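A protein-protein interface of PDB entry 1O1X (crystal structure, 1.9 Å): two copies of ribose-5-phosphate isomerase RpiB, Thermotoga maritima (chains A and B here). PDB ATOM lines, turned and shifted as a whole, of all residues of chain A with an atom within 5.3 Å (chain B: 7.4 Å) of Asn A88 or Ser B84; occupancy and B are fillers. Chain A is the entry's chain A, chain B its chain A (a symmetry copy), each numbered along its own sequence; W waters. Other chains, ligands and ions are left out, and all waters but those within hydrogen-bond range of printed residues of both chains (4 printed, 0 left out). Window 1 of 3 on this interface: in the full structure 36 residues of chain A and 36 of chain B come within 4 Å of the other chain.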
ATOM      1  N   MET A  83      -0.320 -16.208  21.544  1.00  0.00           N
ATOM      2  CA  MET A  83       0.718 -16.699  20.662  1.00  0.00           C
ATOM      3  C   MET A  83       1.030 -18.178  20.875  1.00  0.00           C
ATOM      4  O   MET A  83       1.208 -18.945  19.888  1.00  0.00           O
ATOM      5  CB  MET A  83       2.005 -15.895  20.814  1.00  0.00           C
ATOM      6  CG  MET A  83       1.972 -14.485  20.281  1.00  0.00           C
ATOM      7  SD  MET A  83       1.371 -14.371  18.373  1.00  0.00           S
ATOM      8  CE  MET A  83       1.845 -12.458  18.031  1.00  0.00           C
ATOM      9  N   SER A  84       1.085 -18.601  22.129  1.00  0.00           N
ATOM     10  CA  SER A  84       1.349 -20.008  22.452  1.00  0.00           C
ATOM     11  C   SER A  84       0.214 -20.917  21.882  1.00  0.00           C
ATOM     12  O   SER A  84       0.484 -22.015  21.379  1.00  0.00           O
ATOM     13  CB  SER A  84       1.566 -20.258  23.941  1.00  0.00           C
ATOM     14  OG  SER A  84       0.392 -20.128  24.695  1.00  0.00           O
ATOM     15  N   ILE A  85      -1.016 -20.422  21.896  1.00  0.00           N
ATOM     16  CA  ILE A  85      -2.146 -21.154  21.331  1.00  0.00           C
ATOM     17  C   ILE A  85      -2.109 -21.122  19.799  1.00  0.00           C
ATOM     18  O   ILE A  85      -2.128 -22.158  19.151  1.00  0.00           O
ATOM     19  CB  ILE A  85      -3.470 -20.622  21.872  1.00  0.00           C
ATOM     20  CG1 ILE A  85      -3.588 -20.836  23.400  1.00  0.00           C
ATOM     21  CG2 ILE A  85      -4.653 -21.319  21.229  1.00  0.00           C
ATOM     22  CD1 ILE A  85      -4.575 -19.922  24.063  1.00  0.00           C
ATOM     23  N   ALA A  86      -2.011 -19.937  19.215  1.00  0.00           N
ATOM     24  CA  ALA A  86      -2.104 -19.799  17.765  1.00  0.00           C
ATOM     25  C   ALA A  86      -1.005 -20.517  17.003  1.00  0.00           C
ATOM     26  O   ALA A  86      -1.270 -21.186  15.999  1.00  0.00           O
ATOM     27  CB  ALA A  86      -2.140 -18.326  17.378  1.00  0.00           C
ATOM     28  N   ALA A  87       0.235 -20.413  17.489  1.00  0.00           N
ATOM     29  CA  ALA A  87       1.376 -20.971  16.778  1.00  0.00           C
ATOM     30  C   ALA A  87       1.382 -22.489  16.841  1.00  0.00           C
ATOM     31  O   ALA A  87       1.787 -23.139  15.885  1.00  0.00           O
ATOM     32  CB  ALA A  87       2.705 -20.366  17.277  1.00  0.00           C
ATOM     33  N   ASN A  88       0.907 -23.049  17.943  1.00  0.00           N
ATOM     34  CA  ASN A  88       0.940 -24.494  18.123  1.00  0.00           C
ATOM     35  C   ASN A  88      -0.193 -25.245  17.398  1.00  0.00           C
ATOM     36  O   ASN A  88      -0.316 -26.462  17.478  1.00  0.00           O
ATOM     37  CB  ASN A  88       0.994 -24.793  19.605  1.00  0.00           C
ATOM     38  CG  ASN A  88       2.393 -24.565  20.185  1.00  0.00           C
ATOM     39  OD1 ASN A  88       3.404 -24.997  19.578  1.00  0.00           O
ATOM     40  ND2 ASN A  88       2.455 -23.922  21.344  1.00  0.00           N
ATOM     41  N   ARG A  89      -1.010 -24.512  16.647  1.00  0.00           N
ATOM     42  CA  ARG A  89      -1.983 -25.099  15.722  1.00  0.00           C
ATOM     43  C   ARG A  89      -1.319 -25.856  14.577  1.00  0.00           C
ATOM     44  O   ARG A  89      -1.950 -26.691  13.945  1.00  0.00           O
ATOM     45  CB  ARG A  89      -2.886 -24.013  15.151  1.00  0.00           C
ATOM     46  CG  ARG A  89      -3.982 -23.575  16.094  1.00  0.00           C
ATOM     47  CD  ARG A  89      -5.061 -24.638  16.272  1.00  0.00           C
ATOM     48  NE  ARG A  89      -6.217 -24.082  16.953  1.00  0.00           N
ATOM     49  CZ  ARG A  89      -6.349 -23.959  18.283  1.00  0.00           C
ATOM     50  NH1 ARG A  89      -5.399 -24.353  19.119  1.00  0.00           N
ATOM     51  NH2 ARG A  89      -7.456 -23.419  18.771  1.00  0.00           N
ATOM     52  N   TYR A  90      -0.047 -25.553  14.319  1.00  0.00           N
ATOM     53  CA  TYR A  90       0.639 -26.050  13.130  1.00  0.00           C
ATOM     54  C   TYR A  90       1.566 -27.207  13.440  1.00  0.00           C
ATOM     55  O   TYR A  90       2.462 -27.095  14.294  1.00  0.00           O
ATOM     56  CB  TYR A  90       1.405 -24.905  12.481  1.00  0.00           C
ATOM     57  CG  TYR A  90       0.465 -23.826  12.026  1.00  0.00           C
ATOM     58  CD1 TYR A  90      -0.164 -23.915  10.791  1.00  0.00           C
ATOM     59  CD2 TYR A  90       0.174 -22.745  12.845  1.00  0.00           C
ATOM     60  CE1 TYR A  90      -1.067 -22.966  10.405  1.00  0.00           C
ATOM     61  CE2 TYR A  90      -0.706 -21.783  12.464  1.00  0.00           C
ATOM     62  CZ  TYR A  90      -1.332 -21.904  11.251  1.00  0.00           C
ATOM     63  OH  TYR A  90      -2.178 -20.938  10.843  1.00  0.00           O
ATOM     64  N   ILE A  93       5.533 -27.134  14.544  1.00  0.00           N
ATOM     65  CA  ILE A  93       5.832 -25.971  15.361  1.00  0.00           C
ATOM     66  C   ILE A  93       5.764 -26.353  16.810  1.00  0.00           C
ATOM     67  O   ILE A  93       4.805 -26.986  17.253  1.00  0.00           O
ATOM     68  CB  ILE A  93       4.821 -24.806  15.071  1.00  0.00           C
ATOM     69  CG1 ILE A  93       4.915 -24.373  13.606  1.00  0.00           C
ATOM     70  CG2 ILE A  93       5.010 -23.641  16.075  1.00  0.00           C
ATOM     71  CD1 ILE A  93       6.276 -23.766  13.174  1.00  0.00           C
ATOM     72  N   ARG A  94       6.803 -25.990  17.557  1.00  0.00           N
ATOM     73  CA  ARG A  94       6.836 -26.195  19.009  1.00  0.00           C
ATOM     74  C   ARG A  94       7.175 -24.838  19.633  1.00  0.00           C
ATOM     75  O   ARG A  94       8.323 -24.439  19.736  1.00  0.00           O
ATOM     76  CB  ARG A  94       7.813 -27.308  19.334  1.00  0.00           C
ATOM     77  CG  ARG A  94       7.349 -28.695  18.839  1.00  0.00           C
ATOM     78  CD  ARG A  94       8.317 -29.840  19.129  1.00  0.00           C
ATOM     79  NE  ARG A  94       9.576 -29.554  18.481  1.00  0.00           N
ATOM     80  CZ  ARG A  94       9.844 -29.721  17.194  1.00  0.00           C
ATOM     81  NH1 ARG A  94       8.981 -30.268  16.371  1.00  0.00           N
ATOM     82  NH2 ARG A  94      11.002 -29.289  16.726  1.00  0.00           N
ATOM     83  N   ALA A  95       6.111 -24.094  19.961  1.00  0.00           N
ATOM     84  CA  ALA A  95       6.198 -22.760  20.492  1.00  0.00           C
ATOM     85  C   ALA A  95       6.065 -22.789  22.005  1.00  0.00           C
ATOM     86  O   ALA A  95       5.033 -23.255  22.558  1.00  0.00           O
ATOM     87  CB  ALA A  95       5.114 -21.882  19.866  1.00  0.00           C
ATOM     88  N   ALA A  96       7.086 -22.265  22.690  1.00  0.00           N
ATOM     89  CA  ALA A  96       7.209 -22.393  24.141  1.00  0.00           C
ATOM     90  C   ALA A  96       7.143 -21.029  24.832  1.00  0.00           C
ATOM     91  O   ALA A  96       8.032 -20.193  24.671  1.00  0.00           O
ATOM     92  CB  ALA A  96       8.529 -23.080  24.510  1.00  0.00           C
ATOM     93  N   TYR B  54       3.634 -37.319  27.440  1.00  0.00           N
ATOM     94  CA  TYR B  54       2.601 -36.290  27.632  1.00  0.00           C
ATOM     95  C   TYR B  54       1.553 -36.158  26.484  1.00  0.00           C
ATOM     96  O   TYR B  54       0.381 -35.912  26.797  1.00  0.00           O
ATOM     97  CB  TYR B  54       3.216 -34.893  28.005  1.00  0.00           C
ATOM     98  CG  TYR B  54       4.194 -34.301  27.012  1.00  0.00           C
ATOM     99  CD1 TYR B  54       3.762 -33.556  25.907  1.00  0.00           C
ATOM    100  CD2 TYR B  54       5.556 -34.465  27.181  1.00  0.00           C
ATOM    101  CE1 TYR B  54       4.687 -33.048  24.968  1.00  0.00           C
ATOM    102  CE2 TYR B  54       6.493 -33.951  26.257  1.00  0.00           C
ATOM    103  CZ  TYR B  54       6.051 -33.230  25.155  1.00  0.00           C
ATOM    104  OH  TYR B  54       6.993 -32.727  24.265  1.00  0.00           O
ATOM    105  N   ALA B  58      -2.664 -35.370  26.733  1.00  0.00           N
ATOM    106  CA  ALA B  58      -3.254 -34.197  26.096  1.00  0.00           C
ATOM    107  C   ALA B  58      -4.460 -34.608  25.243  1.00  0.00           C
ATOM    108  O   ALA B  58      -5.523 -33.987  25.340  1.00  0.00           O
ATOM    109  CB  ALA B  58      -2.214 -33.460  25.233  1.00  0.00           C
ATOM    110  N   LEU B  75      -4.343 -29.845  32.255  1.00  0.00           N
ATOM    111  CA  LEU B  75      -3.242 -30.681  31.807  1.00  0.00           C
ATOM    112  C   LEU B  75      -1.984 -30.244  32.527  1.00  0.00           C
ATOM    113  O   LEU B  75      -1.718 -29.040  32.702  1.00  0.00           O
ATOM    114  CB  LEU B  75      -3.043 -30.560  30.294  1.00  0.00           C
ATOM    115  CG  LEU B  75      -4.107 -31.231  29.405  1.00  0.00           C
ATOM    116  CD1 LEU B  75      -3.881 -30.897  27.923  1.00  0.00           C
ATOM    117  CD2 LEU B  75      -4.089 -32.754  29.669  1.00  0.00           C
ATOM    118  N   OCS B  77       2.323 -31.196  32.958  1.00  0.00           N
ATOM    119  CA  OCS B  77       3.595 -31.909  32.842  1.00  0.00           C
ATOM    120  CB  OCS B  77       3.924 -32.223  31.382  1.00  0.00           C
ATOM    121  SG  OCS B  77       4.380 -30.864  30.270  1.00  0.00           S
ATOM    122  C   OCS B  77       4.660 -31.152  33.612  1.00  0.00           C
ATOM    123  O   OCS B  77       4.339 -30.235  34.352  1.00  0.00           O
ATOM    124  OD1 OCS B  77       5.610 -30.325  30.779  1.00  0.00           O
ATOM    125  OD2 OCS B  77       4.674 -31.449  29.075  1.00  0.00           O
ATOM    126  OD3 OCS B  77       3.384 -29.954  30.074  1.00  0.00           O
ATOM    127  N   THR B  79       6.980 -28.858  33.080  1.00  0.00           N
ATOM    128  CA  THR B  79       7.053 -27.427  32.904  1.00  0.00           C
ATOM    129  C   THR B  79       5.790 -26.840  32.355  1.00  0.00           C
ATOM    130  O   THR B  79       5.657 -25.602  32.252  1.00  0.00           O
ATOM    131  CB  THR B  79       8.185 -27.074  31.922  1.00  0.00           C
ATOM    132  OG1 THR B  79       7.886 -27.672  30.638  1.00  0.00           O
ATOM    133  CG2 THR B  79       9.527 -27.617  32.391  1.00  0.00           C
ATOM    134  N   GLY B  80       4.891 -27.695  31.880  1.00  0.00           N
ATOM    135  CA  GLY B  80       3.724 -27.208  31.159  1.00  0.00           C
ATOM    136  C   GLY B  80       3.927 -27.029  29.675  1.00  0.00           C
ATOM    137  O   GLY B  80       2.947 -26.972  28.921  1.00  0.00           O
ATOM    138  N   LEU B  81       5.170 -26.993  29.215  1.00  0.00           N
ATOM    139  CA  LEU B  81       5.432 -26.653  27.820  1.00  0.00           C
ATOM    140  C   LEU B  81       4.899 -27.713  26.854  1.00  0.00           C
ATOM    141  O   LEU B  81       4.216 -27.378  25.897  1.00  0.00           O
ATOM    142  CB  LEU B  81       6.909 -26.407  27.611  1.00  0.00           C
ATOM    143  CG  LEU B  81       7.451 -25.156  28.362  1.00  0.00           C
ATOM    144  CD1 LEU B  81       8.938 -25.110  28.245  1.00  0.00           C
ATOM    145  CD2 LEU B  81       6.836 -23.895  27.863  1.00  0.00           C
ATOM    146  N   GLY B  82       5.208 -28.981  27.106  1.00  0.00           N
ATOM    147  CA  GLY B  82       4.751 -30.089  26.279  1.00  0.00           C
ATOM    148  C   GLY B  82       3.248 -30.133  26.108  1.00  0.00           C
ATOM    149  O   GLY B  82       2.765 -30.249  24.990  1.00  0.00           O
ATOM    150  N   MET B  83       2.520 -29.952  27.200  1.00  0.00           N
ATOM    151  CA  MET B  83       1.073 -29.917  27.181  1.00  0.00           C
ATOM    152  C   MET B  83       0.516 -28.709  26.430  1.00  0.00           C
ATOM    153  O   MET B  83      -0.465 -28.837  25.646  1.00  0.00           O
ATOM    154  CB  MET B  83       0.495 -29.930  28.592  1.00  0.00           C
ATOM    155  CG  MET B  83       0.631 -31.227  29.350  1.00  0.00           C
ATOM    156  SD  MET B  83      -0.087 -32.809  28.352  1.00  0.00           S
ATOM    157  CE  MET B  83      -0.039 -34.141  29.844  1.00  0.00           C
ATOM    158  N   SER B  84       1.123 -27.550  26.634  1.00  0.00           N
ATOM    159  CA  SER B  84       0.693 -26.328  25.943  1.00  0.00           C
ATOM    160  C   SER B  84       0.868 -26.487  24.400  1.00  0.00           C
ATOM    161  O   SER B  84       0.017 -26.036  23.623  1.00  0.00           O
ATOM    162  CB  SER B  84       1.384 -25.067  26.454  1.00  0.00           C
ATOM    163  OG  SER B  84       2.736 -25.000  26.092  1.00  0.00           O
ATOM    164  N   ILE B  85       1.915 -27.186  23.983  1.00  0.00           N
ATOM    165  CA  ILE B  85       2.146 -27.455  22.567  1.00  0.00           C
ATOM    166  C   ILE B  85       1.178 -28.524  22.048  1.00  0.00           C
ATOM    167  O   ILE B  85       0.464 -28.304  21.081  1.00  0.00           O
ATOM    168  CB  ILE B  85       3.600 -27.843  22.312  1.00  0.00           C
ATOM    169  CG1 ILE B  85       4.567 -26.684  22.653  1.00  0.00           C
ATOM    170  CG2 ILE B  85       3.831 -28.205  20.858  1.00  0.00           C
ATOM    171  CD1 ILE B  85       5.974 -27.129  22.917  1.00  0.00           C
ATOM    172  N   ALA B  86       1.117 -29.668  22.713  1.00  0.00           N
ATOM    173  CA  ALA B  86       0.327 -30.790  22.216  1.00  0.00           C
ATOM    174  C   ALA B  86      -1.162 -30.504  22.121  1.00  0.00           C
ATOM    175  O   ALA B  86      -1.805 -30.847  21.124  1.00  0.00           O
ATOM    176  CB  ALA B  86       0.574 -32.027  23.069  1.00  0.00           C
ATOM    177  N   ALA B  87      -1.717 -29.847  23.142  1.00  0.00           N
ATOM    178  CA  ALA B  87      -3.154 -29.617  23.203  1.00  0.00           C
ATOM    179  C   ALA B  87      -3.595 -28.584  22.180  1.00  0.00           C
ATOM    180  O   ALA B  87      -4.684 -28.696  21.631  1.00  0.00           O
ATOM    181  CB  ALA B  87      -3.608 -29.249  24.631  1.00  0.00           C
ATOM    182  N   ASN B  88      -2.745 -27.607  21.905  1.00  0.00           N
ATOM    183  CA  ASN B  88      -3.111 -26.532  20.992  1.00  0.00           C
ATOM    184  C   ASN B  88      -2.983 -26.901  19.502  1.00  0.00           C
ATOM    185  O   ASN B  88      -3.227 -26.092  18.613  1.00  0.00           O
ATOM    186  CB  ASN B  88      -2.323 -25.295  21.365  1.00  0.00           C
ATOM    187  CG  ASN B  88      -2.895 -24.604  22.605  1.00  0.00           C
ATOM    188  OD1 ASN B  88      -4.134 -24.425  22.710  1.00  0.00           O
ATOM    189  ND2 ASN B  88      -2.018 -24.201  23.516  1.00  0.00           N
ATOM    190  N   ARG B  89      -2.633 -28.154  19.224  1.00  0.00           N
ATOM    191  CA  ARG B  89      -2.694 -28.717  17.873  1.00  0.00           C
ATOM    192  C   ARG B  89      -4.119 -28.808  17.340  1.00  0.00           C
ATOM    193  O   ARG B  89      -4.321 -28.900  16.138  1.00  0.00           O
ATOM    194  CB  ARG B  89      -2.058 -30.102  17.853  1.00  0.00           C
ATOM    195  CG  ARG B  89      -0.549 -30.079  17.822  1.00  0.00           C
ATOM    196  CD  ARG B  89       0.003 -29.603  16.482  1.00  0.00           C
ATOM    197  NE  ARG B  89       1.431 -29.856  16.400  1.00  0.00           N
ATOM    198  CZ  ARG B  89       2.390 -29.058  16.893  1.00  0.00           C
ATOM    199  NH1 ARG B  89       2.104 -27.926  17.518  1.00  0.00           N
ATOM    200  NH2 ARG B  89       3.657 -29.419  16.758  1.00  0.00           N
ATOM    201  N   TYR B  90      -5.098 -28.783  18.245  1.00  0.00           N
ATOM    202  CA  TYR B  90      -6.485 -29.068  17.889  1.00  0.00           C
ATOM    203  C   TYR B  90      -7.321 -27.810  17.779  1.00  0.00           C
ATOM    204  O   TYR B  90      -7.399 -27.010  18.728  1.00  0.00           O
ATOM    205  CB  TYR B  90      -7.079 -30.021  18.918  1.00  0.00           C
ATOM    206  CG  TYR B  90      -6.348 -31.333  18.912  1.00  0.00           C
ATOM    207  CD1 TYR B  90      -6.692 -32.326  18.004  1.00  0.00           C
ATOM    208  CD2 TYR B  90      -5.291 -31.561  19.780  1.00  0.00           C
ATOM    209  CE1 TYR B  90      -5.985 -33.493  17.958  1.00  0.00           C
ATOM    210  CE2 TYR B  90      -4.593 -32.726  19.759  1.00  0.00           C
ATOM    211  CZ  TYR B  90      -4.935 -33.683  18.839  1.00  0.00           C
ATOM    212  OH  TYR B  90      -4.278 -34.859  18.831  1.00  0.00           O
ATOM    213  N   ILE B  93      -9.461 -25.848  20.700  1.00  0.00           N
ATOM    214  CA  ILE B  93      -8.803 -25.946  21.991  1.00  0.00           C
ATOM    215  C   ILE B  93      -7.974 -24.716  22.219  1.00  0.00           C
ATOM    216  O   ILE B  93      -7.208 -24.300  21.349  1.00  0.00           O
ATOM    217  CB  ILE B  93      -7.891 -27.221  22.062  1.00  0.00           C
ATOM    218  CG1 ILE B  93      -8.733 -28.487  21.880  1.00  0.00           C
ATOM    219  CG2 ILE B  93      -7.037 -27.226  23.355  1.00  0.00           C
ATOM    220  CD1 ILE B  93      -9.788 -28.754  22.987  1.00  0.00           C
ATOM    221  N   ALA B  95      -5.557 -23.898  25.158  1.00  0.00           N
ATOM    222  CA  ALA B  95      -4.870 -24.372  26.330  1.00  0.00           C
ATOM    223  C   ALA B  95      -3.843 -23.348  26.785  1.00  0.00           C
ATOM    224  O   ALA B  95      -2.905 -22.986  26.026  1.00  0.00           O
ATOM    225  CB  ALA B  95      -4.205 -25.715  26.034  1.00  0.00           C
ATOM    226  N   ALA B  96      -3.987 -22.894  28.035  1.00  0.00           N
ATOM    227  CA  ALA B  96      -3.214 -21.769  28.557  1.00  0.00           C
ATOM    228  C   ALA B  96      -2.309 -22.199  29.714  1.00  0.00           C
ATOM    229  O   ALA B  96      -2.785 -22.575  30.785  1.00  0.00           O
ATOM    230  CB  ALA B  96      -4.148 -20.653  29.038  1.00  0.00           C
ATOM    231  N   LEU B  97      -1.012 -22.071  29.499  1.00  0.00           N
ATOM    232  CA  LEU B  97       0.032 -22.340  30.494  1.00  0.00           C
ATOM    233  C   LEU B  97       0.086 -21.127  31.444  1.00  0.00           C
ATOM    234  O   LEU B  97       0.496 -20.019  31.044  1.00  0.00           O
ATOM    235  CB  LEU B  97       1.362 -22.554  29.765  1.00  0.00           C
ATOM    236  CG  LEU B  97       2.620 -22.789  30.597  1.00  0.00           C
ATOM    237  CD1 LEU B  97       2.391 -23.808  31.655  1.00  0.00           C
ATOM    238  CD2 LEU B  97       3.834 -23.155  29.723  1.00  0.00           C
ATOM    239  N   VAL B 117      -3.199 -25.242  31.714  1.00  0.00           N
ATOM    240  CA  VAL B 117      -2.004 -26.040  31.784  1.00  0.00           C
ATOM    241  C   VAL B 117      -1.151 -25.541  32.951  1.00  0.00           C
ATOM    242  O   VAL B 117      -0.871 -24.328  33.070  1.00  0.00           O
ATOM    243  CB  VAL B 117      -1.191 -25.976  30.437  1.00  0.00           C
ATOM    244  CG1 VAL B 117       0.107 -26.768  30.549  1.00  0.00           C
ATOM    245  CG2 VAL B 117      -2.038 -26.436  29.252  1.00  0.00           C
HETATM  246  O   HOH W   1      -4.707 -27.203  13.905  1.00  0.00           O
HETATM  247  O   HOH W   2      -0.383 -21.938  26.475  1.00  0.00           O
HETATM  248  O   HOH W   3      -2.527 -29.460  14.056  1.00  0.00           O
HETATM  249  O   HOH W   4       3.830 -22.834  25.016  1.00  0.00           O
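The backbone carbonyl oxygen (O) of Asn A88 lies within hydrogen-bond range of the guanidinium group (NH1) of Arg B89.
O of Asn B88 sits close to O of Asn A88 (3.1 Å).
The guanidinium group (NH2) of Arg B89 is in hydrogen-bond range of the backbone carbonyl oxygen (O) of Ile A93, 2.7 Å away.
The backbone carbonyl oxygen of Tyr A90 lies close to the guanidinium group of Arg B89 (3.3 Å).
O of Ile B93 sits at hydrogen-bond distance from NH2 of Arg A89, at 2.7 Å.
The backbone carbonyl oxygen (O) of Tyr B90 sits close to the guanidinium group (NH1) of Arg A89.
NH1 of Arg A89 sits at hydrogen-bond distance from O of Asn B88, at 2.8 Å.
Water W2 lies within hydrogen-bond range of OG of Ser A84 (2.7 Å), O of Ala B95 (2.8 Å) and N of Leu B97 (3.1 Å).
Water W4 bridges OG of Ser B84 (2.7 Å) and O of Ala A95 (2.8 Å).
Water W3 lies within hydrogen-bond range of O of Arg B89 (2.8 Å) and O of Arg A89 (2.8 Å).
Water W1 lies within hydrogen-bond range of the backbone carbonyl oxygen of Arg A89 (2.8 Å) and the backbone carbonyl oxygen of Arg B89 (2.8 Å).
OG1 of Thr B79 sits at hydrogen-bond distance from N of Leu B81 (3.1 Å).
O of Ser A84 is in hydrogen-bond range of ND2 of Asn A88, at 2.7 Å.
OD1 of Asn B88 sits at hydrogen-bond distance from N of Ala B95, at 2.9 Å.
The backbone carbonyl oxygen of Gly B80 is in hydrogen-bond range of the side-chain hydroxyl of Ser B84 (3.5 Å).
OD1 of Asn B88 sits close to O of Ile B93 (3.4 Å).
The backbone carbonyl oxygen of Ser B84 is in hydrogen-bond range of the side-chain amide nitrogen of Asn B88, at 2.7 Å.
Asn B88 touches Ser A84 (ND2 to O, 3.95 Å).
CG2 of Ile A85 touches OD1 of Asn B88 (3.5 Å).
CG2 of Ile A85 touches O of Ile B93 (3.9 Å).
Ala B95 touches Ile A85 (O to CG1, 3.5 Å).
Ser B84 touches Asn A88.
Asn A88 touches Ile B85.
Arg A89 touches Arg B89 (O to O, 3.9 Å).
Ile B85 touches Ile A93 (CG2 to O, 3.9 Å).
O of Ala A95 touches CG1 of Ile B85, 3.5 Å away.
Leu B81 touches Ala A96.
Of the 21 printed residues of chain B, 8 touch a printed residue of chain A.
Hydrophobic or aromatic side chains of chain B within 4 Å of the printed part of chain A: Leu B81 and Ile B85.
Of the 12 printed residues of chain A, 8 touch a printed residue of chain B.
Hydrophobic or aromatic side chains of chain A that line the printed part of chain B: Ile A85 and Ala A96.
Among the printed residues, no Asp or Glu carboxylate lies within 4 Å of a Lys or Arg side-chain nitrogen of the other chain.
Ser A84 touches Asn B88, and with the chains exchanged Asn A88 touches Ser B84.
Asn A88 touches Arg B89, and with the chains exchanged Arg A89 touches Asn B88.
Arg A89 touches its own counterpart, Arg B89.
Arg A89 touches Tyr B90, and with the chains exchanged Tyr A90 touches Arg B89.
Of the printed residues of chain B, Ile A85 touches Asn B88, Ile B93 and Ala B95.
Ala A86 touches none of the printed residues of chain B.
Ala A87 touches none of the printed residues of chain B.
Printed residues of chain B within 4 Å of Ile A93: Ile B85 (3.9 Å) and Arg B89 (2.7 Å).
Of the printed residues of chain B, Ala A95 touches Ile B85 (3.5 Å).
Of the printed residues of chain A, Ser B84 touches Asn A88.
Printed residues of chain A within 4 Å of Tyr B90: Arg A89.
Printed residues of chain A within 4 Å of Ile B93: Ile A85 (3.9 Å) and Arg A89 (2.7 Å).
Leu B97 touches none of the printed residues of chain A.
The nearest printed residue of chain B that does not touch Asn A88 is Tyr B90 (5.4 Å).
The nearest printed residue of chain A that does not touch Ser B84 is Ala A95 (4.6 Å).
The nearest printed residue of chain A that does not touch Ile B85 is Arg A94 (4.03 Å).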
